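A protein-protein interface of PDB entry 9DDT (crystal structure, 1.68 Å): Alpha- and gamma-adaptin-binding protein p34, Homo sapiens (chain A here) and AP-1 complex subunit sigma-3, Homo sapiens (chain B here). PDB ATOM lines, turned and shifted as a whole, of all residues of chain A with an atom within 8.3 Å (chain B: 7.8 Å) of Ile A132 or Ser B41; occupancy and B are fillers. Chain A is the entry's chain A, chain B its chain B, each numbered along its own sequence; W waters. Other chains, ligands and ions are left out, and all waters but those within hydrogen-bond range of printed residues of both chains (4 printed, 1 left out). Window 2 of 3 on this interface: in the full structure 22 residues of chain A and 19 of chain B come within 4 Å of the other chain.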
ATOM      1  N   LYS A 103     -42.555  -2.908   4.516  1.00  0.00           N
ATOM      2  CA  LYS A 103     -42.769  -1.653   5.247  1.00  0.00           C
ATOM      3  C   LYS A 103     -43.690  -1.843   6.450  1.00  0.00           C
ATOM      4  O   LYS A 103     -43.690  -0.996   7.349  1.00  0.00           O
ATOM      5  CB  LYS A 103     -43.337  -0.577   4.309  1.00  0.00           C
ATOM      6  CG  LYS A 103     -42.328  -0.200   3.249  1.00  0.00           C
ATOM      7  CD  LYS A 103     -42.773   0.922   2.301  1.00  0.00           C
ATOM      8  CE  LYS A 103     -41.744   1.178   1.217  1.00  0.00           C
ATOM      9  NZ  LYS A 103     -40.481   1.752   1.828  1.00  0.00           N
ATOM     10  N   LEU A 112     -31.309  -7.453  -0.797  1.00  0.00           N
ATOM     11  CA  LEU A 112     -31.716  -7.881  -2.129  1.00  0.00           C
ATOM     12  C   LEU A 112     -30.579  -8.701  -2.724  1.00  0.00           C
ATOM     13  O   LEU A 112     -29.454  -8.207  -2.829  1.00  0.00           O
ATOM     14  CB  LEU A 112     -32.020  -6.670  -3.017  1.00  0.00           C
ATOM     15  CG  LEU A 112     -32.446  -6.984  -4.445  1.00  0.00           C
ATOM     16  CD1 LEU A 112     -33.853  -7.584  -4.442  1.00  0.00           C
ATOM     17  CD2 LEU A 112     -32.363  -5.711  -5.340  1.00  0.00           C
ATOM     18  N   ARG A 124     -26.621  -2.788 -12.449  1.00  0.00           N
ATOM     19  CA  ARG A 124     -26.272  -2.350 -11.104  1.00  0.00           C
ATOM     20  C   ARG A 124     -26.947  -1.029 -10.761  1.00  0.00           C
ATOM     21  O   ARG A 124     -27.421  -0.853  -9.637  1.00  0.00           O
ATOM     22  CB  ARG A 124     -24.750  -2.242 -10.960  1.00  0.00           C
ATOM     23  CG  ARG A 124     -24.273  -2.088  -9.526  1.00  0.00           C
ATOM     24  CD  ARG A 124     -22.748  -2.095  -9.472  1.00  0.00           C
ATOM     25  NE  ARG A 124     -22.196  -3.358  -9.967  1.00  0.00           N
ATOM     26  CZ  ARG A 124     -22.262  -4.518  -9.314  1.00  0.00           C
ATOM     27  NH1 ARG A 124     -22.827  -4.581  -8.116  1.00  0.00           N
ATOM     28  NH2 ARG A 124     -21.742  -5.612  -9.849  1.00  0.00           N
ATOM     29  N   GLN A 125     -27.012  -0.095 -11.721  1.00  0.00           N
ATOM     30  CA  GLN A 125     -27.634   1.204 -11.468  1.00  0.00           C
ATOM     31  C   GLN A 125     -29.079   1.044 -11.022  1.00  0.00           C
ATOM     32  O   GLN A 125     -29.522   1.666 -10.053  1.00  0.00           O
ATOM     33  CB  GLN A 125     -27.555   2.074 -12.726  1.00  0.00           C
ATOM     34  CG  GLN A 125     -28.246   3.445 -12.632  1.00  0.00           C
ATOM     35  CD  GLN A 125     -27.647   4.372 -11.593  1.00  0.00           C
ATOM     36  OE1 GLN A 125     -28.362   5.137 -10.940  1.00  0.00           O
ATOM     37  NE2 GLN A 125     -26.325   4.324 -11.442  1.00  0.00           N
ATOM     38  N   LYS A 126     -29.824   0.195 -11.713  1.00  0.00           N
ATOM     39  CA  LYS A 126     -31.247   0.074 -11.436  1.00  0.00           C
ATOM     40  C   LYS A 126     -31.482  -0.670 -10.120  1.00  0.00           C
ATOM     41  O   LYS A 126     -32.324  -0.261  -9.298  1.00  0.00           O
ATOM     42  CB  LYS A 126     -31.867  -0.594 -12.654  1.00  0.00           C
ATOM     43  CG  LYS A 126     -33.311  -0.913 -12.712  1.00  0.00           C
ATOM     44  CD  LYS A 126     -33.671  -0.372 -14.097  1.00  0.00           C
ATOM     45  CE  LYS A 126     -32.903  -1.114 -15.191  1.00  0.00           C
ATOM     46  NZ  LYS A 126     -33.160  -0.546 -16.562  1.00  0.00           N
ATOM     47  N   ALA A 127     -30.676  -1.706  -9.857  1.00  0.00           N
ATOM     48  CA  ALA A 127     -30.776  -2.399  -8.574  1.00  0.00           C
ATOM     49  C   ALA A 127     -30.393  -1.479  -7.418  1.00  0.00           C
ATOM     50  O   ALA A 127     -31.039  -1.486  -6.363  1.00  0.00           O
ATOM     51  CB  ALA A 127     -29.897  -3.653  -8.586  1.00  0.00           C
ATOM     52  N   GLN A 128     -29.349  -0.669  -7.604  1.00  0.00           N
ATOM     53  CA  GLN A 128     -28.939   0.265  -6.560  1.00  0.00           C
ATOM     54  C   GLN A 128     -30.017   1.307  -6.299  1.00  0.00           C
ATOM     55  O   GLN A 128     -30.297   1.640  -5.143  1.00  0.00           O
ATOM     56  CB  GLN A 128     -27.631   0.961  -6.948  1.00  0.00           C
ATOM     57  CG  GLN A 128     -26.399   0.136  -6.681  1.00  0.00           C
ATOM     58  CD  GLN A 128     -26.150  -0.028  -5.202  1.00  0.00           C
ATOM     59  OE1 GLN A 128     -26.494  -1.053  -4.625  1.00  0.00           O
ATOM     60  NE2 GLN A 128     -25.583   1.003  -4.569  1.00  0.00           N
ATOM     61  N   GLU A 129     -30.590   1.880  -7.362  1.00  0.00           N
ATOM     62  CA  GLU A 129     -31.661   2.861  -7.197  1.00  0.00           C
ATOM     63  C   GLU A 129     -32.775   2.281  -6.346  1.00  0.00           C
ATOM     64  O   GLU A 129     -33.261   2.919  -5.400  1.00  0.00           O
ATOM     65  CB  GLU A 129     -32.208   3.276  -8.560  1.00  0.00           C
ATOM     66  CG  GLU A 129     -31.294   4.167  -9.366  1.00  0.00           C
ATOM     67  CD  GLU A 129     -31.969   4.697 -10.621  1.00  0.00           C
ATOM     68  OE1 GLU A 129     -33.140   4.322 -10.878  1.00  0.00           O
ATOM     69  OE2 GLU A 129     -31.322   5.475 -11.355  1.00  0.00           O
ATOM     70  N   TRP A 130     -33.163   1.039  -6.650  1.00  0.00           N
ATOM     71  CA  TRP A 130     -34.238   0.408  -5.888  1.00  0.00           C
ATOM     72  C   TRP A 130     -33.831   0.173  -4.431  1.00  0.00           C
ATOM     73  O   TRP A 130     -34.588   0.507  -3.506  1.00  0.00           O
ATOM     74  CB  TRP A 130     -34.656  -0.889  -6.591  1.00  0.00           C
ATOM     75  CG  TRP A 130     -35.855  -1.588  -6.005  1.00  0.00           C
ATOM     76  CD1 TRP A 130     -37.159  -1.515  -6.456  1.00  0.00           C
ATOM     77  CD2 TRP A 130     -35.870  -2.476  -4.884  1.00  0.00           C
ATOM     78  NE1 TRP A 130     -37.971  -2.314  -5.672  1.00  0.00           N
ATOM     79  CE2 TRP A 130     -37.204  -2.907  -4.704  1.00  0.00           C
ATOM     80  CE3 TRP A 130     -34.883  -2.956  -4.015  1.00  0.00           C
ATOM     81  CZ2 TRP A 130     -37.571  -3.784  -3.683  1.00  0.00           C
ATOM     82  CZ3 TRP A 130     -35.250  -3.822  -3.006  1.00  0.00           C
ATOM     83  CH2 TRP A 130     -36.581  -4.234  -2.851  1.00  0.00           C
ATOM     84  N   CYS A 131     -32.613  -0.342  -4.197  1.00  0.00           N
ATOM     85  CA  CYS A 131     -32.170  -0.595  -2.822  1.00  0.00           C
ATOM     86  C   CYS A 131     -32.078   0.671  -1.998  1.00  0.00           C
ATOM     87  O   CYS A 131     -32.490   0.683  -0.833  1.00  0.00           O
ATOM     88  CB  CYS A 131     -30.825  -1.321  -2.781  1.00  0.00           C
ATOM     89  SG  CYS A 131     -30.856  -2.997  -3.439  1.00  0.00           S
ATOM     90  N   ILE A 132     -31.516   1.740  -2.564  1.00  0.00           N
ATOM     91  CA  ILE A 132     -31.372   2.964  -1.790  1.00  0.00           C
ATOM     92  C   ILE A 132     -32.742   3.550  -1.492  1.00  0.00           C
ATOM     93  O   ILE A 132     -33.006   3.999  -0.367  1.00  0.00           O
ATOM     94  CB  ILE A 132     -30.462   3.960  -2.526  1.00  0.00           C
ATOM     95  CG1 ILE A 132     -29.028   3.442  -2.487  1.00  0.00           C
ATOM     96  CG2 ILE A 132     -30.493   5.328  -1.843  1.00  0.00           C
ATOM     97  CD1 ILE A 132     -28.246   3.759  -3.721  1.00  0.00           C
ATOM     98  N   LYS A 133     -33.652   3.507  -2.479  1.00  0.00           N
ATOM     99  CA  LYS A 133     -35.006   3.994  -2.255  1.00  0.00           C
ATOM    100  C   LYS A 133     -35.680   3.253  -1.104  1.00  0.00           C
ATOM    101  O   LYS A 133     -36.383   3.868  -0.291  1.00  0.00           O
ATOM    102  CB  LYS A 133     -35.814   3.858  -3.551  1.00  0.00           C
ATOM    103  CG  LYS A 133     -37.309   4.032  -3.427  1.00  0.00           C
ATOM    104  CD  LYS A 133     -37.929   4.230  -4.822  1.00  0.00           C
ATOM    105  CE  LYS A 133     -39.422   4.533  -4.780  1.00  0.00           C
ATOM    106  NZ  LYS A 133     -40.084   4.133  -6.062  1.00  0.00           N
ATOM    107  N   HIS A 134     -35.457   1.938  -0.994  1.00  0.00           N
ATOM    108  CA  HIS A 134     -36.232   1.134  -0.056  1.00  0.00           C
ATOM    109  C   HIS A 134     -35.473   0.689   1.190  1.00  0.00           C
ATOM    110  O   HIS A 134     -36.062   0.007   2.041  1.00  0.00           O
ATOM    111  CB  HIS A 134     -36.819  -0.072  -0.799  1.00  0.00           C
ATOM    112  CG  HIS A 134     -37.754   0.315  -1.907  1.00  0.00           C
ATOM    113  ND1 HIS A 134     -38.877   1.088  -1.699  1.00  0.00           N
ATOM    114  CD2 HIS A 134     -37.712   0.063  -3.237  1.00  0.00           C
ATOM    115  CE1 HIS A 134     -39.503   1.271  -2.850  1.00  0.00           C
ATOM    116  NE2 HIS A 134     -38.814   0.666  -3.801  1.00  0.00           N
ATOM    117  N   GLY A 135     -34.216   1.086   1.354  1.00  0.00           N
ATOM    118  CA  GLY A 135     -33.470   0.706   2.542  1.00  0.00           C
ATOM    119  C   GLY A 135     -32.830  -0.664   2.489  1.00  0.00           C
ATOM    120  O   GLY A 135     -32.471  -1.209   3.539  1.00  0.00           O
ATOM    121  N   PHE A 136     -32.672  -1.232   1.299  1.00  0.00           N
ATOM    122  CA  PHE A 136     -32.002  -2.509   1.115  1.00  0.00           C
ATOM    123  C   PHE A 136     -30.535  -2.306   0.754  1.00  0.00           C
ATOM    124  O   PHE A 136     -30.093  -1.223   0.350  1.00  0.00           O
ATOM    125  CB  PHE A 136     -32.673  -3.298  -0.009  1.00  0.00           C
ATOM    126  CG  PHE A 136     -33.997  -3.884   0.351  1.00  0.00           C
ATOM    127  CD1 PHE A 136     -35.082  -3.058   0.627  1.00  0.00           C
ATOM    128  CD2 PHE A 136     -34.194  -5.258   0.319  1.00  0.00           C
ATOM    129  CE1 PHE A 136     -36.335  -3.583   0.910  1.00  0.00           C
ATOM    130  CE2 PHE A 136     -35.463  -5.799   0.606  1.00  0.00           C
ATOM    131  CZ  PHE A 136     -36.530  -4.961   0.898  1.00  0.00           C
ATOM    132  N   GLU A 137     -29.791  -3.400   0.843  1.00  0.00           N
ATOM    133  CA  GLU A 137     -28.455  -3.512   0.290  1.00  0.00           C
ATOM    134  C   GLU A 137     -28.442  -4.588  -0.793  1.00  0.00           C
ATOM    135  O   GLU A 137     -29.113  -5.621  -0.661  1.00  0.00           O
ATOM    136  CB  GLU A 137     -27.487  -3.851   1.412  1.00  0.00           C
ATOM    137  CG  GLU A 137     -26.179  -4.308   0.992  1.00  0.00           C
ATOM    138  CD  GLU A 137     -25.355  -4.778   2.179  1.00  0.00           C
ATOM    139  OE1 GLU A 137     -25.772  -4.566   3.353  1.00  0.00           O
ATOM    140  OE2 GLU A 137     -24.295  -5.342   1.915  1.00  0.00           O
ATOM    141  N   LEU A 138     -27.711  -4.338  -1.876  1.00  0.00           N
ATOM    142  CA  LEU A 138     -27.614  -5.288  -2.980  1.00  0.00           C
ATOM    143  C   LEU A 138     -26.449  -6.248  -2.760  1.00  0.00           C
ATOM    144  O   LEU A 138     -25.323  -5.809  -2.509  1.00  0.00           O
ATOM    145  CB  LEU A 138     -27.419  -4.557  -4.308  1.00  0.00           C
ATOM    146  CG  LEU A 138     -27.153  -5.447  -5.529  1.00  0.00           C
ATOM    147  CD1 LEU A 138     -28.376  -6.304  -5.856  1.00  0.00           C
ATOM    148  CD2 LEU A 138     -26.710  -4.606  -6.714  1.00  0.00           C
ATOM    149  N   PHE B   8     -22.146   5.420   8.448  1.00  0.00           N
ATOM    150  CA  PHE B   8     -23.410   4.768   8.083  1.00  0.00           C
ATOM    151  C   PHE B   8     -23.174   3.582   7.153  1.00  0.00           C
ATOM    152  O   PHE B   8     -22.139   3.465   6.509  1.00  0.00           O
ATOM    153  CB  PHE B   8     -24.410   5.747   7.446  1.00  0.00           C
ATOM    154  CG  PHE B   8     -23.881   6.519   6.266  1.00  0.00           C
ATOM    155  CD1 PHE B   8     -23.223   7.730   6.449  1.00  0.00           C
ATOM    156  CD2 PHE B   8     -24.115   6.081   4.971  1.00  0.00           C
ATOM    157  CE1 PHE B   8     -22.776   8.458   5.368  1.00  0.00           C
ATOM    158  CE2 PHE B   8     -23.679   6.804   3.882  1.00  0.00           C
ATOM    159  CZ  PHE B   8     -23.010   7.996   4.074  1.00  0.00           C
ATOM    160  N   ARG B  10     -24.471   0.546   4.097  1.00  0.00           N
ATOM    161  CA  ARG B  10     -25.063   0.474   2.760  1.00  0.00           C
ATOM    162  C   ARG B  10     -26.585   0.425   2.805  1.00  0.00           C
ATOM    163  O   ARG B  10     -27.248   0.812   1.831  1.00  0.00           O
ATOM    164  CB  ARG B  10     -24.536  -0.758   2.025  1.00  0.00           C
ATOM    165  CG  ARG B  10     -23.183  -0.547   1.375  1.00  0.00           C
ATOM    166  CD  ARG B  10     -23.318  -0.345  -0.121  1.00  0.00           C
ATOM    167  NE  ARG B  10     -22.018  -0.391  -0.783  1.00  0.00           N
ATOM    168  CZ  ARG B  10     -21.714   0.281  -1.888  1.00  0.00           C
ATOM    169  NH1 ARG B  10     -20.506   0.166  -2.424  1.00  0.00           N
ATOM    170  NH2 ARG B  10     -22.620   1.065  -2.463  1.00  0.00           N
ATOM    171  N   GLN B  11     -27.162  -0.048   3.913  1.00  0.00           N
ATOM    172  CA  GLN B  11     -28.607  -0.041   4.085  1.00  0.00           C
ATOM    173  C   GLN B  11     -29.125   1.292   4.610  1.00  0.00           C
ATOM    174  O   GLN B  11     -30.322   1.419   4.885  1.00  0.00           O
ATOM    175  CB  GLN B  11     -29.032  -1.173   5.028  1.00  0.00           C
ATOM    176  CG  GLN B  11     -28.967  -2.563   4.373  1.00  0.00           C
ATOM    177  CD  GLN B  11     -29.110  -3.688   5.393  1.00  0.00           C
ATOM    178  OE1 GLN B  11     -30.100  -3.740   6.128  1.00  0.00           O
ATOM    179  NE2 GLN B  11     -28.101  -4.570   5.472  1.00  0.00           N
ATOM    180  N   GLY B  12     -28.251   2.285   4.759  1.00  0.00           N
ATOM    181  CA  GLY B  12     -28.692   3.587   5.205  1.00  0.00           C
ATOM    182  C   GLY B  12     -28.794   3.747   6.698  1.00  0.00           C
ATOM    183  O   GLY B  12     -29.464   4.677   7.168  1.00  0.00           O
ATOM    184  N   GLU B  34     -30.962  12.955   4.493  1.00  0.00           N
ATOM    185  CA  GLU B  34     -30.658  13.476   3.161  1.00  0.00           C
ATOM    186  C   GLU B  34     -29.237  13.115   2.721  1.00  0.00           C
ATOM    187  O   GLU B  34     -29.010  12.686   1.577  1.00  0.00           O
ATOM    188  CB  GLU B  34     -30.851  14.991   3.139  1.00  0.00           C
ATOM    189  CG  GLU B  34     -30.689  15.575   1.755  1.00  0.00           C
ATOM    190  CD  GLU B  34     -31.076  17.027   1.685  1.00  0.00           C
ATOM    191  OE1 GLU B  34     -31.974  17.443   2.453  1.00  0.00           O
ATOM    192  OE2 GLU B  34     -30.483  17.746   0.857  1.00  0.00           O
ATOM    193  N   ILE B  35     -28.262  13.319   3.607  1.00  0.00           N
ATOM    194  CA  ILE B  35     -26.867  13.097   3.241  1.00  0.00           C
ATOM    195  C   ILE B  35     -26.619  11.628   2.935  1.00  0.00           C
ATOM    196  O   ILE B  35     -25.906  11.291   1.978  1.00  0.00           O
ATOM    197  CB  ILE B  35     -25.953  13.622   4.361  1.00  0.00           C
ATOM    198  CG1 ILE B  35     -25.984  15.152   4.345  1.00  0.00           C
ATOM    199  CG2 ILE B  35     -24.535  13.060   4.222  1.00  0.00           C
ATOM    200  CD1 ILE B  35     -24.977  15.788   5.250  1.00  0.00           C
ATOM    201  N   VAL B  36     -27.172  10.738   3.755  1.00  0.00           N
ATOM    202  CA  VAL B  36     -26.990   9.313   3.522  1.00  0.00           C
ATOM    203  C   VAL B  36     -27.535   8.942   2.149  1.00  0.00           C
ATOM    204  O   VAL B  36     -26.865   8.245   1.372  1.00  0.00           O
ATOM    205  CB  VAL B  36     -27.656   8.504   4.649  1.00  0.00           C
ATOM    206  CG1 VAL B  36     -27.765   7.043   4.265  1.00  0.00           C
ATOM    207  CG2 VAL B  36     -26.863   8.662   5.944  1.00  0.00           C
ATOM    208  N   GLN B  37     -28.725   9.456   1.798  1.00  0.00           N
ATOM    209  CA  GLN B  37     -29.254   9.157   0.465  1.00  0.00           C
ATOM    210  C   GLN B  37     -28.315   9.656  -0.626  1.00  0.00           C
ATOM    211  O   GLN B  37     -28.061   8.949  -1.614  1.00  0.00           O
ATOM    212  CB  GLN B  37     -30.630   9.786   0.254  1.00  0.00           C
ATOM    213  CG  GLN B  37     -31.306   9.350  -1.081  1.00  0.00           C
ATOM    214  CD  GLN B  37     -30.872  10.125  -2.336  1.00  0.00           C
ATOM    215  OE1 GLN B  37     -30.355  11.244  -2.267  1.00  0.00           O
ATOM    216  NE2 GLN B  37     -31.105   9.519  -3.504  1.00  0.00           N
ATOM    217  N   ILE B  38     -27.811  10.886  -0.483  1.00  0.00           N
ATOM    218  CA  ILE B  38     -26.954  11.445  -1.530  1.00  0.00           C
ATOM    219  C   ILE B  38     -25.711  10.587  -1.718  1.00  0.00           C
ATOM    220  O   ILE B  38     -25.337  10.243  -2.850  1.00  0.00           O
ATOM    221  CB  ILE B  38     -26.580  12.903  -1.218  1.00  0.00           C
ATOM    222  CG1 ILE B  38     -27.811  13.803  -1.400  1.00  0.00           C
ATOM    223  CG2 ILE B  38     -25.412  13.334  -2.087  1.00  0.00           C
ATOM    224  CD1 ILE B  38     -27.697  15.151  -0.728  1.00  0.00           C
ATOM    225  N   ILE B  39     -25.039  10.250  -0.613  1.00  0.00           N
ATOM    226  CA  ILE B  39     -23.763   9.556  -0.730  1.00  0.00           C
ATOM    227  C   ILE B  39     -23.969   8.131  -1.246  1.00  0.00           C
ATOM    228  O   ILE B  39     -23.226   7.666  -2.125  1.00  0.00           O
ATOM    229  CB  ILE B  39     -23.003   9.593   0.607  1.00  0.00           C
ATOM    230  CG1 ILE B  39     -22.505  11.030   0.847  1.00  0.00           C
ATOM    231  CG2 ILE B  39     -21.838   8.616   0.575  1.00  0.00           C
ATOM    232  CD1 ILE B  39     -21.964  11.255   2.252  1.00  0.00           C
ATOM    233  N   LEU B  40     -24.981   7.423  -0.730  1.00  0.00           N
ATOM    234  CA  LEU B  40     -25.209   6.048  -1.177  1.00  0.00           C
ATOM    235  C   LEU B  40     -25.478   5.989  -2.677  1.00  0.00           C
ATOM    236  O   LEU B  40     -25.108   5.007  -3.339  1.00  0.00           O
ATOM    237  CB  LEU B  40     -26.386   5.436  -0.406  1.00  0.00           C
ATOM    238  CG  LEU B  40     -26.134   5.086   1.066  1.00  0.00           C
ATOM    239  CD1 LEU B  40     -27.303   4.298   1.661  1.00  0.00           C
ATOM    240  CD2 LEU B  40     -24.820   4.309   1.229  1.00  0.00           C
ATOM    241  N   SER B  41     -26.083   7.038  -3.238  1.00  0.00           N
ATOM    242  CA  SER B  41     -26.463   7.051  -4.648  1.00  0.00           C
ATOM    243  C   SER B  41     -25.311   7.367  -5.585  1.00  0.00           C
ATOM    244  O   SER B  41     -25.482   7.269  -6.801  1.00  0.00           O
ATOM    245  CB  SER B  41     -27.591   8.057  -4.884  1.00  0.00           C
ATOM    246  OG  SER B  41     -28.675   7.772  -4.023  1.00  0.00           O
ATOM    247  N   ARG B  42     -24.146   7.740  -5.066  1.00  0.00           N
ATOM    248  CA  ARG B  42     -23.020   8.047  -5.937  1.00  0.00           C
ATOM    249  C   ARG B  42     -22.360   6.742  -6.366  1.00  0.00           C
ATOM    250  O   ARG B  42     -21.746   6.047  -5.550  1.00  0.00           O
ATOM    251  CB  ARG B  42     -22.053   8.984  -5.228  1.00  0.00           C
ATOM    252  CG  ARG B  42     -22.652  10.361  -5.162  1.00  0.00           C
ATOM    253  CD  ARG B  42     -21.790  11.305  -4.418  1.00  0.00           C
ATOM    254  NE  ARG B  42     -20.582  11.677  -5.145  1.00  0.00           N
ATOM    255  CZ  ARG B  42     -20.496  12.711  -5.976  1.00  0.00           C
ATOM    256  NH1 ARG B  42     -21.561  13.471  -6.213  1.00  0.00           N
ATOM    257  NH2 ARG B  42     -19.346  12.972  -6.583  1.00  0.00           N
ATOM    258  N   GLY B  43     -22.491   6.406  -7.644  1.00  0.00           N
ATOM    259  CA  GLY B  43     -21.966   5.147  -8.128  1.00  0.00           C
ATOM    260  C   GLY B  43     -20.558   5.240  -8.672  1.00  0.00           C
ATOM    261  O   GLY B  43     -19.880   4.221  -8.831  1.00  0.00           O
ATOM    262  N   HIS B  44     -20.102   6.454  -8.964  1.00  0.00           N
ATOM    263  CA  HIS B  44     -18.779   6.681  -9.526  1.00  0.00           C
ATOM    264  C   HIS B  44     -18.006   7.636  -8.636  1.00  0.00           C
ATOM    265  O   HIS B  44     -18.520   8.690  -8.253  1.00  0.00           O
ATOM    266  CB  HIS B  44     -18.873   7.230 -10.943  1.00  0.00           C
ATOM    267  CG  HIS B  44     -19.541   6.289 -11.888  1.00  0.00           C
ATOM    268  ND1 HIS B  44     -19.003   5.063 -12.216  1.00  0.00           N
ATOM    269  CD2 HIS B  44     -20.733   6.360 -12.524  1.00  0.00           C
ATOM    270  CE1 HIS B  44     -19.817   4.435 -13.046  1.00  0.00           C
ATOM    271  NE2 HIS B  44     -20.875   5.201 -13.250  1.00  0.00           N
ATOM    272  N   TYR B  59     -16.062  12.081   1.859  1.00  0.00           N
ATOM    273  CA  TYR B  59     -16.498  10.763   2.295  1.00  0.00           C
ATOM    274  C   TYR B  59     -15.634   9.697   1.658  1.00  0.00           C
ATOM    275  O   TYR B  59     -14.991   9.916   0.624  1.00  0.00           O
ATOM    276  CB  TYR B  59     -17.981  10.518   1.977  1.00  0.00           C
ATOM    277  CG  TYR B  59     -18.232  10.236   0.513  1.00  0.00           C
ATOM    278  CD1 TYR B  59     -18.396  11.280  -0.392  1.00  0.00           C
ATOM    279  CD2 TYR B  59     -18.294   8.928   0.025  1.00  0.00           C
ATOM    280  CE1 TYR B  59     -18.619  11.044  -1.737  1.00  0.00           C
ATOM    281  CE2 TYR B  59     -18.502   8.686  -1.330  1.00  0.00           C
ATOM    282  CZ  TYR B  59     -18.660   9.744  -2.198  1.00  0.00           C
ATOM    283  OH  TYR B  59     -18.876   9.531  -3.543  1.00  0.00           O
ATOM    284  N   TYR B  66     -19.639   3.725   5.356  1.00  0.00           N
ATOM    285  CA  TYR B  66     -19.264   5.017   4.807  1.00  0.00           C
ATOM    286  C   TYR B  66     -18.878   5.942   5.948  1.00  0.00           C
ATOM    287  O   TYR B  66     -19.568   5.984   6.973  1.00  0.00           O
ATOM    288  CB  TYR B  66     -20.406   5.646   4.010  1.00  0.00           C
ATOM    289  CG  TYR B  66     -20.586   5.009   2.666  1.00  0.00           C
ATOM    290  CD1 TYR B  66     -21.255   3.799   2.545  1.00  0.00           C
ATOM    291  CD2 TYR B  66     -20.047   5.586   1.530  1.00  0.00           C
ATOM    292  CE1 TYR B  66     -21.408   3.200   1.315  1.00  0.00           C
ATOM    293  CE2 TYR B  66     -20.194   4.992   0.293  1.00  0.00           C
ATOM    294  CZ  TYR B  66     -20.877   3.802   0.199  1.00  0.00           C
ATOM    295  OH  TYR B  66     -21.035   3.201  -1.034  1.00  0.00           O
HETATM  296  O   HOH W   1     -25.594  -2.366   5.222  1.00  0.00           O
HETATM  297  O   HOH W   2     -32.369  -1.975   6.117  1.00  0.00           O
HETATM  298  O   HOH W   3     -24.869   3.563  -5.756  1.00  0.00           O
HETATM  299  O   HOH W   4     -24.674   2.355  -2.070  1.00  0.00           O
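Among the printed residues, pairs that only touch across the chains: Gln A128 with Arg B10 (3.6 Å), Ile A132 with Leu B40 (3.4 Å), Ile A132 with Ser B41 (3.7 Å), Gly A135 with Gln B11 (3.7 Å), Phe A136 with Arg B10 (3.8 Å) and Phe A136 with Gln B11 (3.95 Å).
Hydrophobic or aromatic side chains of chain A within 4 Å of the printed part of chain B: Ile A132.
Of the 17 printed residues of chain B, 4 touch a printed residue of chain A.
Among the printed residues, no Asp or Glu carboxylate lies within 4 Å of a Lys or Arg side-chain nitrogen of the other chain.
Of chain B, only Leu B40 and Ser B41 come within 4 Å of Ile A132.
Of chain A, only Ile A132 (3.7 Å) comes within 4 Å of Ser B41.
Of the printed residues of chain B, Gln A128 touches Arg B10 (3.6 Å).
Of the printed residues of chain B, Phe A136 touches Arg B10 and Gln B11.
Water W4 lies within hydrogen-bond range of the guanidinium group of Arg B10, the backbone carbonyl oxygen of Leu B40 and the side-chain amide nitrogen of Gln A128.
Water W2 bridges the backbone carbonyl oxygen of Gly A135 (2.7 Å) and the side-chain amide oxygen of Gln B11 (2.9 Å).
Water W3 bridges O of Leu B40 and NE2 of Gln A128.
Water W1 lies within hydrogen-bond range of OE1 of Glu A137, N of Gln B11 and N of Arg B10.
The backbone carbonyl oxygen (O) of Glu A137 lies within hydrogen-bond range of the backbone NH (N) of Leu A112 (2.9 Å).
The backbone carbonyl oxygen of Cys A131 is in hydrogen-bond range of the backbone NH of Phe A136, 2.9 Å away.
NH2 of Arg B10 sits at hydrogen-bond distance from OH of Tyr B66.
OG of Ser B41 sits at hydrogen-bond distance from O of Gln B37, 2.8 Å away.
OE1 of Glu A137 lies within hydrogen-bond range of NE2 of Gln B11, at 3.1 Å.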
